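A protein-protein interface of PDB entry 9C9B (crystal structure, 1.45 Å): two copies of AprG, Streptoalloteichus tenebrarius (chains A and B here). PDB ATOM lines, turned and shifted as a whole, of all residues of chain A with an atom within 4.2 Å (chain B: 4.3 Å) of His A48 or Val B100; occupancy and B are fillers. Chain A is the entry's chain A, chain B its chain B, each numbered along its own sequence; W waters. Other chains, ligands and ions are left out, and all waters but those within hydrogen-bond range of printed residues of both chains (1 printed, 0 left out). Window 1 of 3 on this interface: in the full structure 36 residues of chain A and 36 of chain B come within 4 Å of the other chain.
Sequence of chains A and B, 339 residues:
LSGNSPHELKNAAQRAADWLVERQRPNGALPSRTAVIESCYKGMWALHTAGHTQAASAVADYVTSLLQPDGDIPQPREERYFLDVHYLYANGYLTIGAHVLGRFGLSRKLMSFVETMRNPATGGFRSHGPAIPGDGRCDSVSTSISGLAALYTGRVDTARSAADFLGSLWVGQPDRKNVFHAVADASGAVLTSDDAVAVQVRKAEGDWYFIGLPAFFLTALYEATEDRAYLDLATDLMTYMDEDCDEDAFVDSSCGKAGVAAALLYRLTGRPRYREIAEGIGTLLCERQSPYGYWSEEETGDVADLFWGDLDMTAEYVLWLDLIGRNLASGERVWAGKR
Water W1 lies within hydrogen-bond range of O of Val A100 and OH of Tyr B152.
NE2 of His A48 sits at hydrogen-bond distance from NE2 of His B48 (2.8 Å).
His A48 touches its own counterpart, His B48. His A48 touches Val B100, but with the chains exchanged Val A100 does not touch His B48 (5.3 Å). Positions printed for both chains: 48, 100 and 101. Of the 2 pairs that touch across the chains among the printed residues, 1 has its exchanged pair printed and touching as well.
His A48 touches Val B100.
Of the printed residues of chain B, His A48 touches His B48 and Val B100. Of the printed residues of chain A, His B48 touches His A48. Printed residues of chain A within 4 Å of Val B100: His A48 (3.8 Å). Gly B102 touches none of the printed residues of chain A. The nearest printed residue of chain B that does not touch His A48 is Tyr B152 (7.3 Å).
Of the 12 printed residues of chain A, 1 touches a printed residue of chain B. Printed residues of chain A that touch a printed residue of chain B: His A48. Hydrophobic or aromatic side chains of chain A within 4 Å of the printed part of chain B: His A48. Along chain B the printed residues that touch a printed residue of chain A span positions 48 to 100. Among the printed residues, no Asp or Glu carboxylate lies within 4 Å of a Lys or Arg side-chain nitrogen of the other chain.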
ATOM      1  N   MET A  44      19.072 -24.088  26.860  1.00  0.00           N
ATOM      2  CA  MET A  44      20.288 -23.309  26.627  1.00  0.00           C
ATOM      3  C   MET A  44      20.025 -21.821  26.808  1.00  0.00           C
ATOM      4  O   MET A  44      20.766 -21.125  27.513  1.00  0.00           O
ATOM      5  CB  MET A  44      20.813 -23.564  25.214  1.00  0.00           C
ATOM      6  CG  MET A  44      21.639 -24.822  25.077  1.00  0.00           C
ATOM      7  SD  MET A  44      22.322 -24.967  23.405  1.00  0.00           S
ATOM      8  CE  MET A  44      20.820 -25.253  22.453  1.00  0.00           C
ATOM      9  N   TRP A  45      18.977 -21.313  26.155  1.00  0.00           N
ATOM     10  CA  TRP A  45      18.691 -19.884  26.211  1.00  0.00           C
ATOM     11  C   TRP A  45      18.237 -19.473  27.609  1.00  0.00           C
ATOM     12  O   TRP A  45      18.726 -18.483  28.163  1.00  0.00           O
ATOM     13  CB  TRP A  45      17.639 -19.545  25.161  1.00  0.00           C
ATOM     14  CG  TRP A  45      17.451 -18.073  24.906  1.00  0.00           C
ATOM     15  CD1 TRP A  45      18.263 -17.047  25.306  1.00  0.00           C
ATOM     16  CD2 TRP A  45      16.375 -17.480  24.178  1.00  0.00           C
ATOM     17  NE1 TRP A  45      17.747 -15.839  24.861  1.00  0.00           N
ATOM     18  CE2 TRP A  45      16.590 -16.085  24.171  1.00  0.00           C
ATOM     19  CE3 TRP A  45      15.259 -17.996  23.522  1.00  0.00           C
ATOM     20  CZ2 TRP A  45      15.719 -15.198  23.531  1.00  0.00           C
ATOM     21  CZ3 TRP A  45      14.395 -17.124  22.897  1.00  0.00           C
ATOM     22  CH2 TRP A  45      14.627 -15.736  22.909  1.00  0.00           C
ATOM     23  N   ALA A  46      17.326 -20.245  28.212  1.00  0.00           N
ATOM     24  CA  ALA A  46      16.835 -19.901  29.545  1.00  0.00           C
ATOM     25  C   ALA A  46      17.965 -19.879  30.563  1.00  0.00           C
ATOM     26  O   ALA A  46      18.070 -18.949  31.373  1.00  0.00           O
ATOM     27  CB  ALA A  46      15.758 -20.898  29.986  1.00  0.00           C
ATOM     28  N   LEU A  47      18.812 -20.909  30.556  1.00  0.00           N
ATOM     29  CA  LEU A  47      19.842 -20.985  31.581  1.00  0.00           C
ATOM     30  C   LEU A  47      20.909 -19.924  31.371  1.00  0.00           C
ATOM     31  O   LEU A  47      21.450 -19.386  32.344  1.00  0.00           O
ATOM     32  CB  LEU A  47      20.452 -22.385  31.631  1.00  0.00           C
ATOM     33  CG  LEU A  47      19.474 -23.425  32.177  1.00  0.00           C
ATOM     34  CD1 LEU A  47      20.099 -24.802  32.003  1.00  0.00           C
ATOM     35  CD2 LEU A  47      19.145 -23.161  33.647  1.00  0.00           C
ATOM     36  N   HIS A  48      21.214 -19.602  30.112  1.00  0.00           N
ATOM     37  CA  HIS A  48      22.158 -18.524  29.841  1.00  0.00           C
ATOM     38  C   HIS A  48      21.618 -17.200  30.371  1.00  0.00           C
ATOM     39  O   HIS A  48      22.340 -16.437  31.029  1.00  0.00           O
ATOM     40  CB  HIS A  48      22.450 -18.467  28.338  1.00  0.00           C
ATOM     41  CG  HIS A  48      23.331 -17.326  27.922  1.00  0.00           C
ATOM     42  ND1 HIS A  48      24.686 -17.290  28.165  1.00  0.00           N
ATOM     43  CD2 HIS A  48      23.039 -16.181  27.261  1.00  0.00           C
ATOM     44  CE1 HIS A  48      25.192 -16.172  27.672  1.00  0.00           C
ATOM     45  NE2 HIS A  48      24.214 -15.483  27.117  1.00  0.00           N
ATOM     46  N   THR A  49      20.330 -16.935  30.146  1.00  0.00           N
ATOM     47  CA  THR A  49      19.732 -15.704  30.635  1.00  0.00           C
ATOM     48  C   THR A  49      19.801 -15.608  32.162  1.00  0.00           C
ATOM     49  O   THR A  49      19.892 -14.509  32.725  1.00  0.00           O
ATOM     50  CB  THR A  49      18.313 -15.640  30.074  1.00  0.00           C
ATOM     51  OG1 THR A  49      18.369 -15.890  28.657  1.00  0.00           O
ATOM     52  CG2 THR A  49      17.780 -14.308  30.248  1.00  0.00           C
ATOM     53  N   ALA A  50      19.764 -16.750  32.849  1.00  0.00           N
ATOM     54  CA  ALA A  50      19.869 -16.756  34.297  1.00  0.00           C
ATOM     55  C   ALA A  50      21.310 -16.719  34.796  1.00  0.00           C
ATOM     56  O   ALA A  50      21.531 -16.768  36.009  1.00  0.00           O
ATOM     57  CB  ALA A  50      19.167 -17.993  34.855  1.00  0.00           C
ATOM     58  N   GLY A  51      22.292 -16.627  33.905  1.00  0.00           N
ATOM     59  CA  GLY A  51      23.675 -16.628  34.328  1.00  0.00           C
ATOM     60  C   GLY A  51      24.270 -17.999  34.544  1.00  0.00           C
ATOM     61  O   GLY A  51      25.441 -18.091  34.923  1.00  0.00           O
ATOM     62  N   THR A  53      25.769 -20.358  32.948  1.00  0.00           N
ATOM     63  CA  THR A  53      26.378 -20.602  31.645  1.00  0.00           C
ATOM     64  C   THR A  53      27.036 -21.975  31.557  1.00  0.00           C
ATOM     65  O   THR A  53      27.098 -22.560  30.470  1.00  0.00           O
ATOM     66  CB  THR A  53      27.387 -19.495  31.344  1.00  0.00           C
ATOM     67  OG1 THR A  53      28.274 -19.371  32.457  1.00  0.00           O
ATOM     68  CG2 THR A  53      26.667 -18.154  31.141  1.00  0.00           C
ATOM     69  N   ALA A  56      24.066 -24.124  30.941  1.00  0.00           N
ATOM     70  CA  ALA A  56      23.615 -23.909  29.570  1.00  0.00           C
ATOM     71  C   ALA A  56      24.542 -24.592  28.575  1.00  0.00           C
ATOM     72  O   ALA A  56      24.082 -25.201  27.600  1.00  0.00           O
ATOM     73  CB  ALA A  56      23.548 -22.410  29.290  1.00  0.00           C
ATOM     74  N   VAL A 100      23.535 -17.523  21.159  1.00  0.00           N
ATOM     75  CA  VAL A 100      23.848 -16.575  22.231  1.00  0.00           C
ATOM     76  C   VAL A 100      24.974 -17.094  23.120  1.00  0.00           C
ATOM     77  O   VAL A 100      25.722 -16.301  23.702  1.00  0.00           O
ATOM     78  CB  VAL A 100      22.599 -16.161  23.039  1.00  0.00           C
ATOM     79  CG1 VAL A 100      21.540 -15.548  22.121  1.00  0.00           C
ATOM     80  CG2 VAL A 100      22.050 -17.339  23.841  1.00  0.00           C
ATOM     81  N   LEU A 101      25.128 -18.419  23.228  1.00  0.00           N
ATOM     82  CA  LEU A 101      26.255 -19.014  23.933  1.00  0.00           C
ATOM     83  C   LEU A 101      27.555 -18.943  23.146  1.00  0.00           C
ATOM     84  O   LEU A 101      28.601 -19.321  23.679  1.00  0.00           O
ATOM     85  CB  LEU A 101      25.968 -20.494  24.197  1.00  0.00           C
ATOM     86  CG  LEU A 101      25.220 -20.828  25.480  1.00  0.00           C
ATOM     87  CD1 LEU A 101      24.881 -22.311  25.523  1.00  0.00           C
ATOM     88  CD2 LEU A 101      26.022 -20.434  26.709  1.00  0.00           C
ATOM     89  N   HIS B  48      25.253  -9.626  31.183  1.00  0.00           N
ATOM     90  CA  HIS B  48      24.328 -10.623  30.655  1.00  0.00           C
ATOM     91  C   HIS B  48      24.839 -12.029  30.937  1.00  0.00           C
ATOM     92  O   HIS B  48      24.080 -12.915  31.355  1.00  0.00           O
ATOM     93  CB  HIS B  48      24.124 -10.411  29.152  1.00  0.00           C
ATOM     94  CG  HIS B  48      23.323 -11.492  28.500  1.00  0.00           C
ATOM     95  ND1 HIS B  48      21.946 -11.477  28.448  1.00  0.00           N
ATOM     96  CD2 HIS B  48      23.706 -12.638  27.890  1.00  0.00           C
ATOM     97  CE1 HIS B  48      21.516 -12.562  27.828  1.00  0.00           C
ATOM     98  NE2 HIS B  48      22.565 -13.279  27.474  1.00  0.00           N
ATOM     99  N   ILE B  96      28.582  -6.821  20.393  1.00  0.00           N
ATOM    100  CA  ILE B  96      28.304  -8.163  20.910  1.00  0.00           C
ATOM    101  C   ILE B  96      27.294  -8.103  22.046  1.00  0.00           C
ATOM    102  O   ILE B  96      26.307  -8.849  22.066  1.00  0.00           O
ATOM    103  CB  ILE B  96      29.607  -8.854  21.347  1.00  0.00           C
ATOM    104  CG1 ILE B  96      30.510  -9.077  20.127  1.00  0.00           C
ATOM    105  CG2 ILE B  96      29.306 -10.170  22.086  1.00  0.00           C
ATOM    106  CD1 ILE B  96      31.930  -9.427  20.486  1.00  0.00           C
ATOM    107  N   GLY B  97      27.525  -7.213  23.014  1.00  0.00           N
ATOM    108  CA  GLY B  97      26.618  -7.116  24.146  1.00  0.00           C
ATOM    109  C   GLY B  97      25.209  -6.742  23.726  1.00  0.00           C
ATOM    110  O   GLY B  97      24.229  -7.317  24.214  1.00  0.00           O
ATOM    111  N   ALA B  98      25.086  -5.792  22.798  1.00  0.00           N
ATOM    112  CA  ALA B  98      23.762  -5.417  22.320  1.00  0.00           C
ATOM    113  C   ALA B  98      23.074  -6.591  21.633  1.00  0.00           C
ATOM    114  O   ALA B  98      21.879  -6.838  21.844  1.00  0.00           O
ATOM    115  CB  ALA B  98      23.886  -4.238  21.356  1.00  0.00           C
ATOM    116  N   HIS B  99      23.817  -7.337  20.817  1.00  0.00           N
ATOM    117  CA  HIS B  99      23.203  -8.403  20.045  1.00  0.00           C
ATOM    118  C   HIS B  99      22.720  -9.532  20.941  1.00  0.00           C
ATOM    119  O   HIS B  99      21.608 -10.038  20.763  1.00  0.00           O
ATOM    120  CB  HIS B  99      24.178  -8.944  19.003  1.00  0.00           C
ATOM    121  CG  HIS B  99      23.508  -9.782  17.967  1.00  0.00           C
ATOM    122  ND1 HIS B  99      22.824  -9.232  16.902  1.00  0.00           N
ATOM    123  CD2 HIS B  99      23.338 -11.121  17.873  1.00  0.00           C
ATOM    124  CE1 HIS B  99      22.311 -10.201  16.165  1.00  0.00           C
ATOM    125  NE2 HIS B  99      22.603 -11.357  16.735  1.00  0.00           N
ATOM    126  N   VAL B 100      23.547  -9.950  21.906  1.00  0.00           N
ATOM    127  CA  VAL B 100      23.161 -11.058  22.778  1.00  0.00           C
ATOM    128  C   VAL B 100      21.946 -10.694  23.626  1.00  0.00           C
ATOM    129  O   VAL B 100      21.157 -11.569  24.009  1.00  0.00           O
ATOM    130  CB  VAL B 100      24.368 -11.524  23.618  1.00  0.00           C
ATOM    131  CG1 VAL B 100      23.973 -12.650  24.552  1.00  0.00           C
ATOM    132  CG2 VAL B 100      25.495 -11.990  22.708  1.00  0.00           C
ATOM    133  N   LEU B 101      21.768  -9.406  23.931  1.00  0.00           N
ATOM    134  CA  LEU B 101      20.582  -8.931  24.633  1.00  0.00           C
ATOM    135  C   LEU B 101      19.351  -8.867  23.737  1.00  0.00           C
ATOM    136  O   LEU B 101      18.257  -8.567  24.234  1.00  0.00           O
ATOM    137  CB  LEU B 101      20.829  -7.534  25.201  1.00  0.00           C
ATOM    138  CG  LEU B 101      21.584  -7.412  26.523  1.00  0.00           C
ATOM    139  CD1 LEU B 101      21.962  -5.949  26.775  1.00  0.00           C
ATOM    140  CD2 LEU B 101      20.750  -7.971  27.677  1.00  0.00           C
ATOM    141  N   GLY B 102      19.496  -9.112  22.435  1.00  0.00           N
ATOM    142  CA  GLY B 102      18.377  -8.959  21.537  1.00  0.00           C
ATOM    143  C   GLY B 102      18.069  -7.530  21.158  1.00  0.00           C
ATOM    144  O   GLY B 102      16.996  -7.273  20.603  1.00  0.00           O
ATOM    145  N   TYR B 152      29.094 -12.807  16.023  1.00  0.00           N
ATOM    146  CA  TYR B 152      27.875 -12.709  16.817  1.00  0.00           C
ATOM    147  C   TYR B 152      26.706 -12.144  16.029  1.00  0.00           C
ATOM    148  O   TYR B 152      25.562 -12.539  16.267  1.00  0.00           O
ATOM    149  CB  TYR B 152      28.126 -11.912  18.093  1.00  0.00           C
ATOM    150  CG  TYR B 152      28.618 -12.807  19.209  1.00  0.00           C
ATOM    151  CD1 TYR B 152      27.716 -13.526  19.995  1.00  0.00           C
ATOM    152  CD2 TYR B 152      29.976 -12.940  19.477  1.00  0.00           C
ATOM    153  CE1 TYR B 152      28.166 -14.357  21.012  1.00  0.00           C
ATOM    154  CE2 TYR B 152      30.433 -13.761  20.487  1.00  0.00           C
ATOM    155  CZ  TYR B 152      29.522 -14.465  21.257  1.00  0.00           C
ATOM    156  OH  TYR B 152      29.967 -15.292  22.265  1.00  0.00           O
HETATM  157  O   HOH W   1      28.221 -15.496  24.645  1.00  0.00           O
